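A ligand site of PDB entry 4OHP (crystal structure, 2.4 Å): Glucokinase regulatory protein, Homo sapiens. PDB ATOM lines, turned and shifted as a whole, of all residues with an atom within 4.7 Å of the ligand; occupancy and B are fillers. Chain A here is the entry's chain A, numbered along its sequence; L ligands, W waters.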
ATOM      1  N   VAL A  22      -9.144  -5.361   5.544  1.00  0.00           N
ATOM      2  CA  VAL A  22      -9.527  -5.334   6.944  1.00  0.00           C
ATOM      3  C   VAL A  22      -8.908  -6.530   7.642  1.00  0.00           C
ATOM      4  O   VAL A  22      -9.048  -7.620   7.155  1.00  0.00           O
ATOM      5  CB  VAL A  22     -11.074  -5.369   7.077  1.00  0.00           C
ATOM      6  CG1 VAL A  22     -11.492  -5.610   8.515  1.00  0.00           C
ATOM      7  CG2 VAL A  22     -11.674  -4.074   6.606  1.00  0.00           C
ATOM      8  N   TYR A  36      -2.490  -8.670  15.922  1.00  0.00           N
ATOM      9  CA  TYR A  36      -3.572  -7.744  15.603  1.00  0.00           C
ATOM     10  C   TYR A  36      -3.319  -6.413  16.315  1.00  0.00           C
ATOM     11  O   TYR A  36      -3.316  -5.378  15.670  1.00  0.00           O
ATOM     12  CB  TYR A  36      -4.957  -8.290  16.004  1.00  0.00           C
ATOM     13  CG  TYR A  36      -6.104  -7.383  15.636  1.00  0.00           C
ATOM     14  CD1 TYR A  36      -6.423  -6.246  16.391  1.00  0.00           C
ATOM     15  CD2 TYR A  36      -6.862  -7.638  14.517  1.00  0.00           C
ATOM     16  CE1 TYR A  36      -7.469  -5.397  16.037  1.00  0.00           C
ATOM     17  CE2 TYR A  36      -7.910  -6.818  14.175  1.00  0.00           C
ATOM     18  CZ  TYR A  36      -8.215  -5.695  14.940  1.00  0.00           C
ATOM     19  OH  TYR A  36      -9.290  -4.883  14.552  1.00  0.00           O
ATOM     20  N   GLU A  37      -3.118  -6.465  17.633  1.00  0.00           N
ATOM     21  CA  GLU A  37      -2.879  -5.246  18.450  1.00  0.00           C
ATOM     22  C   GLU A  37      -1.726  -4.424  17.898  1.00  0.00           C
ATOM     23  O   GLU A  37      -1.846  -3.198  17.822  1.00  0.00           O
ATOM     24  CB  GLU A  37      -2.591  -5.608  19.906  1.00  0.00           C
ATOM     25  CG  GLU A  37      -3.516  -4.975  20.951  1.00  0.00           C
ATOM     26  CD  GLU A  37      -4.971  -5.444  20.889  1.00  0.00           C
ATOM     27  OE1 GLU A  37      -5.407  -6.294  21.698  1.00  0.00           O
ATOM     28  OE2 GLU A  37      -5.710  -4.922  20.030  1.00  0.00           O
ATOM     29  N   VAL A  40      -2.770  -2.057  15.074  1.00  0.00           N
ATOM     30  CA  VAL A  40      -3.715  -0.967  15.311  1.00  0.00           C
ATOM     31  C   VAL A  40      -2.921   0.328  15.375  1.00  0.00           C
ATOM     32  O   VAL A  40      -2.059   0.494  16.243  1.00  0.00           O
ATOM     33  CB  VAL A  40      -4.569  -1.118  16.576  1.00  0.00           C
ATOM     34  CG1 VAL A  40      -5.552   0.050  16.691  1.00  0.00           C
ATOM     35  CG2 VAL A  40      -5.311  -2.458  16.577  1.00  0.00           C
ATOM     36  N   PRO A  41      -3.218   1.267  14.457  1.00  0.00           N
ATOM     37  CA  PRO A  41      -2.539   2.551  14.559  1.00  0.00           C
ATOM     38  C   PRO A  41      -2.565   3.159  15.952  1.00  0.00           C
ATOM     39  O   PRO A  41      -3.532   2.993  16.709  1.00  0.00           O
ATOM     40  CB  PRO A  41      -3.338   3.429  13.591  1.00  0.00           C
ATOM     41  CG  PRO A  41      -3.834   2.478  12.532  1.00  0.00           C
ATOM     42  CD  PRO A  41      -4.139   1.210  13.292  1.00  0.00           C
ATOM     43  N   THR A  43      -3.080   5.957  16.908  1.00  0.00           N
ATOM     44  CA  THR A  43      -4.086   6.996  17.034  1.00  0.00           C
ATOM     45  C   THR A  43      -5.475   6.387  17.273  1.00  0.00           C
ATOM     46  O   THR A  43      -6.371   7.067  17.765  1.00  0.00           O
ATOM     47  CB  THR A  43      -4.112   7.929  15.803  1.00  0.00           C
ATOM     48  OG1 THR A  43      -4.338   7.187  14.578  1.00  0.00           O
ATOM     49  CG2 THR A  43      -2.787   8.686  15.684  1.00  0.00           C
ATOM     50  N   GLU A  44      -5.639   5.116  16.898  1.00  0.00           N
ATOM     51  CA  GLU A  44      -6.867   4.394  17.143  1.00  0.00           C
ATOM     52  C   GLU A  44      -6.821   3.500  18.349  1.00  0.00           C
ATOM     53  O   GLU A  44      -7.845   2.980  18.720  1.00  0.00           O
ATOM     54  CB  GLU A  44      -7.209   3.518  15.923  1.00  0.00           C
ATOM     55  CG  GLU A  44      -7.387   4.339  14.647  1.00  0.00           C
ATOM     56  CD  GLU A  44      -8.683   5.130  14.583  1.00  0.00           C
ATOM     57  OE1 GLU A  44      -9.665   4.698  15.191  1.00  0.00           O
ATOM     58  OE2 GLU A  44      -8.730   6.197  13.913  1.00  0.00           O
ATOM     59  N   LYS A  45      -5.664   3.302  18.962  1.00  0.00           N
ATOM     60  CA  LYS A  45      -5.549   2.312  20.035  1.00  0.00           C
ATOM     61  C   LYS A  45      -6.365   2.655  21.270  1.00  0.00           C
ATOM     62  O   LYS A  45      -6.622   3.816  21.567  1.00  0.00           O
ATOM     63  CB  LYS A  45      -4.078   2.047  20.462  1.00  0.00           C
ATOM     64  CG  LYS A  45      -3.273   1.055  19.592  1.00  0.00           C
ATOM     65  CD  LYS A  45      -2.046   0.471  20.297  1.00  0.00           C
ATOM     66  CE  LYS A  45      -0.781   0.411  19.391  1.00  0.00           C
ATOM     67  NZ  LYS A  45      -0.705  -0.618  18.280  1.00  0.00           N
ATOM     68  N   SER A  46      -6.759   1.589  21.952  1.00  0.00           N
ATOM     69  CA  SER A  46      -7.240   1.637  23.312  1.00  0.00           C
ATOM     70  C   SER A  46      -6.048   1.993  24.191  1.00  0.00           C
ATOM     71  O   SER A  46      -5.059   1.290  24.209  1.00  0.00           O
ATOM     72  CB  SER A  46      -7.785   0.231  23.707  1.00  0.00           C
ATOM     73  OG  SER A  46      -8.047   0.107  25.089  1.00  0.00           O
ATOM     74  N   GLY A 193      -3.854  11.102  12.296  1.00  0.00           N
ATOM     75  CA  GLY A 193      -3.834   9.672  12.098  1.00  0.00           C
ATOM     76  C   GLY A 193      -3.127   9.347  10.822  1.00  0.00           C
ATOM     77  O   GLY A 193      -3.033   8.188  10.458  1.00  0.00           O
ATOM     78  N   LEU A 194      -2.607  10.377  10.160  1.00  0.00           N
ATOM     79  CA  LEU A 194      -2.033  10.222   8.835  1.00  0.00           C
ATOM     80  C   LEU A 194      -3.119   9.483   7.985  1.00  0.00           C
ATOM     81  O   LEU A 194      -2.873   8.450   7.403  1.00  0.00           O
ATOM     82  CB  LEU A 194      -0.727   9.476   8.869  1.00  0.00           C
ATOM     83  CG  LEU A 194       0.458  10.086   9.596  1.00  0.00           C
ATOM     84  CD1 LEU A 194       1.712   9.259   9.321  1.00  0.00           C
ATOM     85  CD2 LEU A 194       0.709  11.506   9.136  1.00  0.00           C
ATOM     86  N   SER A 195      -4.289  10.097   7.938  1.00  0.00           N
ATOM     87  CA  SER A 195      -5.497   9.507   7.511  1.00  0.00           C
ATOM     88  C   SER A 195      -6.303  10.309   6.510  1.00  0.00           C
ATOM     89  O   SER A 195      -6.811   9.714   5.586  1.00  0.00           O
ATOM     90  CB  SER A 195      -6.390   9.289   8.709  1.00  0.00           C
ATOM     91  OG  SER A 195      -7.705   9.012   8.272  1.00  0.00           O
ATOM     92  N   ASN A 221       1.379   8.930  13.907  1.00  0.00           N
ATOM     93  CA  ASN A 221       1.630   7.529  13.731  1.00  0.00           C
ATOM     94  C   ASN A 221       2.957   7.342  12.973  1.00  0.00           C
ATOM     95  O   ASN A 221       3.309   8.133  12.119  1.00  0.00           O
ATOM     96  CB  ASN A 221       0.521   6.862  12.899  1.00  0.00           C
ATOM     97  CG  ASN A 221      -0.764   6.674  13.648  1.00  0.00           C
ATOM     98  OD1 ASN A 221      -0.762   6.243  14.810  1.00  0.00           O
ATOM     99  ND2 ASN A 221      -1.892   7.025  13.003  1.00  0.00           N
ATOM    100  N   MET A 225       2.167   2.770   9.934  1.00  0.00           N
ATOM    101  CA  MET A 225       0.777   2.681  10.347  1.00  0.00           C
ATOM    102  C   MET A 225      -0.096   3.710   9.665  1.00  0.00           C
ATOM    103  O   MET A 225      -1.263   3.894  10.041  1.00  0.00           O
ATOM    104  CB  MET A 225       0.682   2.876  11.851  1.00  0.00           C
ATOM    105  CG  MET A 225       1.179   1.713  12.677  1.00  0.00           C
ATOM    106  SD  MET A 225       1.303   2.283  14.386  1.00  0.00           S
ATOM    107  CE  MET A 225       1.412   0.735  15.280  1.00  0.00           C
ATOM    108  N   ALA A 226       0.445   4.423   8.671  1.00  0.00           N
ATOM    109  CA  ALA A 226      -0.336   5.429   7.983  1.00  0.00           C
ATOM    110  C   ALA A 226      -1.477   4.738   7.280  1.00  0.00           C
ATOM    111  O   ALA A 226      -1.335   3.603   6.847  1.00  0.00           O
ATOM    112  CB  ALA A 226       0.520   6.141   6.975  1.00  0.00           C
ATOM    113  N   ARG A 227      -2.585   5.442   7.126  1.00  0.00           N
ATOM    114  CA  ARG A 227      -3.778   4.880   6.475  1.00  0.00           C
ATOM    115  C   ARG A 227      -3.478   4.337   5.062  1.00  0.00           C
ATOM    116  O   ARG A 227      -2.712   4.956   4.303  1.00  0.00           O
ATOM    117  CB  ARG A 227      -4.853   5.935   6.423  1.00  0.00           C
ATOM    118  CG  ARG A 227      -6.207   5.352   6.310  1.00  0.00           C
ATOM    119  CD  ARG A 227      -7.282   6.379   6.584  1.00  0.00           C
ATOM    120  NE  ARG A 227      -8.513   5.894   5.991  1.00  0.00           N
ATOM    121  CZ  ARG A 227      -9.665   6.547   5.964  1.00  0.00           C
ATOM    122  NH1 ARG A 227      -9.799   7.731   6.532  1.00  0.00           N
ATOM    123  NH2 ARG A 227     -10.709   5.965   5.375  1.00  0.00           N
ATOM    124  N   ASP A 229      -6.156   2.189   3.169  1.00  0.00           N
ATOM    125  CA  ASP A 229      -7.318   1.801   2.322  1.00  0.00           C
ATOM    126  C   ASP A 229      -7.498   2.808   1.182  1.00  0.00           C
ATOM    127  O   ASP A 229      -7.110   3.942   1.330  1.00  0.00           O
ATOM    128  CB  ASP A 229      -8.614   1.674   3.129  1.00  0.00           C
ATOM    129  CG  ASP A 229      -8.955   2.949   3.894  1.00  0.00           C
ATOM    130  OD1 ASP A 229      -8.225   3.289   4.856  1.00  0.00           O
ATOM    131  OD2 ASP A 229      -9.973   3.592   3.595  1.00  0.00           O
ATOM    132  N   HIS A 516     -14.123   3.320  24.553  1.00  0.00           N
ATOM    133  CA  HIS A 516     -14.622   3.430  23.193  1.00  0.00           C
ATOM    134  C   HIS A 516     -15.979   4.132  23.192  1.00  0.00           C
ATOM    135  O   HIS A 516     -16.807   3.897  24.076  1.00  0.00           O
ATOM    136  CB  HIS A 516     -14.810   2.031  22.627  1.00  0.00           C
ATOM    137  CG  HIS A 516     -13.530   1.272  22.449  1.00  0.00           C
ATOM    138  ND1 HIS A 516     -12.564   1.672  21.562  1.00  0.00           N
ATOM    139  CD2 HIS A 516     -13.056   0.159  23.046  1.00  0.00           C
ATOM    140  CE1 HIS A 516     -11.546   0.833  21.615  1.00  0.00           C
ATOM    141  NE2 HIS A 516     -11.832  -0.106  22.484  1.00  0.00           N
ATOM    142  N   LYS A 526     -13.419   6.967   7.797  1.00  0.00           N
ATOM    143  CA  LYS A 526     -12.662   6.557   8.999  1.00  0.00           C
ATOM    144  C   LYS A 526     -13.563   6.102  10.149  1.00  0.00           C
ATOM    145  O   LYS A 526     -13.312   5.117  10.844  1.00  0.00           O
ATOM    146  CB  LYS A 526     -11.747   7.689   9.465  1.00  0.00           C
ATOM    147  CG  LYS A 526     -11.100   7.437  10.830  1.00  0.00           C
ATOM    148  CD  LYS A 526     -10.119   8.556  11.125  1.00  0.00           C
ATOM    149  CE  LYS A 526     -10.810   9.892  11.276  1.00  0.00           C
ATOM    150  NZ  LYS A 526      -9.822  10.896  11.704  1.00  0.00           N
ATOM    151  N   TRP A 529     -14.940   2.725   9.284  1.00  0.00           N
ATOM    152  CA  TRP A 529     -13.975   1.659   9.667  1.00  0.00           C
ATOM    153  C   TRP A 529     -13.873   1.484  11.179  1.00  0.00           C
ATOM    154  O   TRP A 529     -13.696   0.368  11.662  1.00  0.00           O
ATOM    155  CB  TRP A 529     -12.611   1.905   9.053  1.00  0.00           C
ATOM    156  CG  TRP A 529     -12.631   1.909   7.570  1.00  0.00           C
ATOM    157  CD1 TRP A 529     -12.254   2.914   6.778  1.00  0.00           C
ATOM    158  CD2 TRP A 529     -13.041   0.844   6.715  1.00  0.00           C
ATOM    159  NE1 TRP A 529     -12.345   2.536   5.468  1.00  0.00           N
ATOM    160  CE2 TRP A 529     -12.867   1.277   5.397  1.00  0.00           C
ATOM    161  CE3 TRP A 529     -13.503  -0.463   6.946  1.00  0.00           C
ATOM    162  CZ2 TRP A 529     -13.167   0.484   4.292  1.00  0.00           C
ATOM    163  CZ3 TRP A 529     -13.804  -1.289   5.846  1.00  0.00           C
ATOM    164  CH2 TRP A 529     -13.647  -0.800   4.532  1.00  0.00           C
ATOM    165  N   ARG A 530     -14.000   2.576  11.925  1.00  0.00           N
ATOM    166  CA  ARG A 530     -13.911   2.490  13.370  1.00  0.00           C
ATOM    167  C   ARG A 530     -15.140   1.748  13.915  1.00  0.00           C
ATOM    168  O   ARG A 530     -15.025   0.955  14.853  1.00  0.00           O
ATOM    169  CB  ARG A 530     -13.722   3.871  14.013  1.00  0.00           C
ATOM    170  CG  ARG A 530     -13.605   3.850  15.546  1.00  0.00           C
ATOM    171  CD  ARG A 530     -13.300   5.239  16.119  1.00  0.00           C
ATOM    172  NE  ARG A 530     -12.182   5.923  15.455  1.00  0.00           N
ATOM    173  CZ  ARG A 530     -12.055   7.249  15.282  1.00  0.00           C
ATOM    174  NH1 ARG A 530     -12.991   8.066  15.726  1.00  0.00           N
ATOM    175  NH2 ARG A 530     -11.000   7.760  14.630  1.00  0.00           N
ATOM    176  N   LEU A 532     -16.731  -0.656  12.335  1.00  0.00           N
ATOM    177  CA  LEU A 532     -16.457  -2.078  12.061  1.00  0.00           C
ATOM    178  C   LEU A 532     -15.454  -2.707  13.067  1.00  0.00           C
ATOM    179  O   LEU A 532     -15.674  -3.794  13.570  1.00  0.00           O
ATOM    180  CB  LEU A 532     -16.003  -2.261  10.613  1.00  0.00           C
ATOM    181  CG  LEU A 532     -15.564  -3.641  10.152  1.00  0.00           C
ATOM    182  CD1 LEU A 532     -16.704  -4.613  10.384  1.00  0.00           C
ATOM    183  CD2 LEU A 532     -15.089  -3.616   8.690  1.00  0.00           C
ATOM    184  N   ALA A 533     -14.375  -2.007  13.350  1.00  0.00           N
ATOM    185  CA  ALA A 533     -13.455  -2.408  14.414  1.00  0.00           C
ATOM    186  C   ALA A 533     -14.118  -2.552  15.769  1.00  0.00           C
ATOM    187  O   ALA A 533     -13.800  -3.493  16.514  1.00  0.00           O
ATOM    188  CB  ALA A 533     -12.317  -1.396  14.554  1.00  0.00           C
ATOM    189  N   GLN A 536     -16.110  -5.809  15.667  1.00  0.00           N
ATOM    190  CA  GLN A 536     -15.237  -7.011  15.814  1.00  0.00           C
ATOM    191  C   GLN A 536     -14.785  -7.186  17.250  1.00  0.00           C
ATOM    192  O   GLN A 536     -14.868  -8.279  17.783  1.00  0.00           O
ATOM    193  CB  GLN A 536     -13.976  -6.928  14.941  1.00  0.00           C
ATOM    194  CG  GLN A 536     -14.252  -6.908  13.467  1.00  0.00           C
ATOM    195  CD  GLN A 536     -13.023  -6.620  12.605  1.00  0.00           C
ATOM    196  OE1 GLN A 536     -12.774  -5.482  12.230  1.00  0.00           O
ATOM    197  NE2 GLN A 536     -12.258  -7.658  12.297  1.00  0.00           N
ATOM    198  N   ARG A 537     -14.326  -6.101  17.871  1.00  0.00           N
ATOM    199  CA  ARG A 537     -13.738  -6.119  19.205  1.00  0.00           C
ATOM    200  C   ARG A 537     -14.740  -6.572  20.277  1.00  0.00           C
ATOM    201  O   ARG A 537     -14.436  -7.442  21.076  1.00  0.00           O
ATOM    202  CB  ARG A 537     -13.127  -4.720  19.520  1.00  0.00           C
ATOM    203  CG  ARG A 537     -12.640  -4.464  20.966  1.00  0.00           C
ATOM    204  CD  ARG A 537     -11.386  -5.212  21.360  1.00  0.00           C
ATOM    205  NE  ARG A 537     -10.208  -4.654  20.688  1.00  0.00           N
ATOM    206  CZ  ARG A 537      -8.971  -5.145  20.736  1.00  0.00           C
ATOM    207  NH1 ARG A 537      -8.688  -6.237  21.432  1.00  0.00           N
ATOM    208  NH2 ARG A 537      -8.012  -4.528  20.072  1.00  0.00           N
HETATM  209  C1  LIG L   1      -7.946  -0.986  20.095  1.00  0.00           C
HETATM  210  N1  LIG L   1      -9.181  -0.447  19.398  1.00  0.00           N
HETATM  211  S1  LIG L   1      -9.390  -1.394  18.260  1.00  0.00           S
HETATM  212  O1  LIG L   1      -8.203  -2.293  18.241  1.00  0.00           O
HETATM  213  O2  LIG L   1     -10.728  -2.127  18.455  1.00  0.00           O
HETATM  214  C2  LIG L   1      -9.386  -0.611  16.746  1.00  0.00           C
HETATM  215  C3  LIG L   1      -8.843  -1.290  15.680  1.00  0.00           C
HETATM  216  C4  LIG L   1      -8.787  -0.721  14.420  1.00  0.00           C
HETATM  217  C5  LIG L   1      -9.889   0.648  16.602  1.00  0.00           C
HETATM  218  C6  LIG L   1      -9.851   1.207  15.355  1.00  0.00           C
HETATM  219  C7  LIG L   1      -9.309   0.537  14.239  1.00  0.00           C
HETATM  220  N2  LIG L   1      -9.283   1.131  12.996  1.00  0.00           N
HETATM  221  C8  LIG L   1      -8.622   0.492  11.856  1.00  0.00           C
HETATM  222  C9  LIG L   1      -8.242   1.507  10.769  1.00  0.00           C
HETATM  223  C10 LIG L   1      -9.656  -0.442  11.320  1.00  0.00           C
HETATM  224  C11 LIG L   1     -10.565  -1.160  10.910  1.00  0.00           C
HETATM  225  C12 LIG L   1     -11.710  -1.983  10.446  1.00  0.00           C
HETATM  226  C13 LIG L   1     -10.233   2.233  12.723  1.00  0.00           C
HETATM  227  C14 LIG L   1      -9.739   3.162  11.587  1.00  0.00           C
HETATM  228  N3  LIG L   1      -9.368   2.374  10.424  1.00  0.00           N
HETATM  229  S2  LIG L   1      -8.940   3.362   9.214  1.00  0.00           S
HETATM  230  O3  LIG L   1      -8.874   2.522   8.003  1.00  0.00           O
HETATM  231  O4  LIG L   1      -9.905   4.479   9.110  1.00  0.00           O
HETATM  232  C15 LIG L   1      -7.392   4.032   9.504  1.00  0.00           C
HETATM  233  C16 LIG L   1      -7.283   5.263  10.144  1.00  0.00           C
HETATM  234  C17 LIG L   1      -6.035   5.781  10.456  1.00  0.00           C
HETATM  235  C18 LIG L   1      -4.941   5.050  10.094  1.00  0.00           C
HETATM  236  N4  LIG L   1      -3.732   5.532  10.359  1.00  0.00           N
HETATM  237  N5  LIG L   1      -5.076   3.868   9.449  1.00  0.00           N
HETATM  238  C19 LIG L   1      -6.250   3.344   9.154  1.00  0.00           C
HETATM  239  O   HOH W   1     -11.123  -4.328  16.493  1.00  0.00           O
HETATM  240  O   HOH W   2      -8.521  -3.891  10.139  1.00  0.00           O
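The guanidinium group (NH2) of Arg 537 lies within hydrogen-bond range of an oxygen (O1) of the ligand (2.9 Å).
O of Gly 193 sits at hydrogen-bond distance from N4 of the ligand, at 2.7 Å.
The backbone carbonyl oxygen (O) of Met 225 lies within hydrogen-bond range of a nitrogen (N4) of the ligand, 3.0 Å away.
The backbone NH (N) of Arg 227 sits close to a nitrogen (N4) of the ligand (3.4 Å).
OD1 of Asp 229 sits close to O3 of the ligand (3.3 Å).
Merely in contact with the ligand: Trp 529, Val 40, Ser 46, Lys 526, His 516, Glu 44, Asn 221, Ala 533, Pro 41, Arg 530, Tyr 36, Ala 226 and Ser 195.
Within 4 Å of the ligand: Tyr 36, Val 40, Pro 41, Glu 44, Ser 46, Gly 193, Ser 195, Asn 221, Met 225, Ala 226, Arg 227, Asp 229, His 516, Lys 526, Trp 529, Arg 530, Ala 533 and Arg 537.
The nearest printed residue that does not touch the ligand is Glu 37 (4.04 Å).
The side-chain carboxylate (OE1) of Glu 44 lies within salt-bridge range of the guanidinium group (NE) of Arg 530 (2.8 Å).
The backbone carbonyl oxygen (O) of Leu 194 lies within hydrogen-bond range of the backbone NH (N) of Arg 227 (3.0 Å).
The backbone carbonyl oxygen of Val 40 lies within hydrogen-bond range of the side-chain amino group of Lys 45.
The guanidinium group of Arg 227 lies within salt-bridge range of the side-chain carboxylate of Asp 229 (2.9 Å).
OG1 of Thr 43 is in hydrogen-bond range of ND2 of Asn 221 (2.9 Å).
The guanidinium group (NH1) of Arg 537 is in salt-bridge range of the side-chain carboxylate (OE1) of Glu 37.
The guanidinium group (NH1) of Arg 227 is in hydrogen-bond range of the side-chain hydroxyl (OG) of Ser 195 (3.0 Å).
The side-chain carboxylate (OD2) of Asp 229 lies within hydrogen-bond range of the indole nitrogen (NE1) of Trp 529, at 3.2 Å.
Water W1 lies within hydrogen-bond range of OH of Tyr 36 (2.7 Å), O of Ala 533 (2.8 Å) and O2 of the ligand (3.0 Å).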
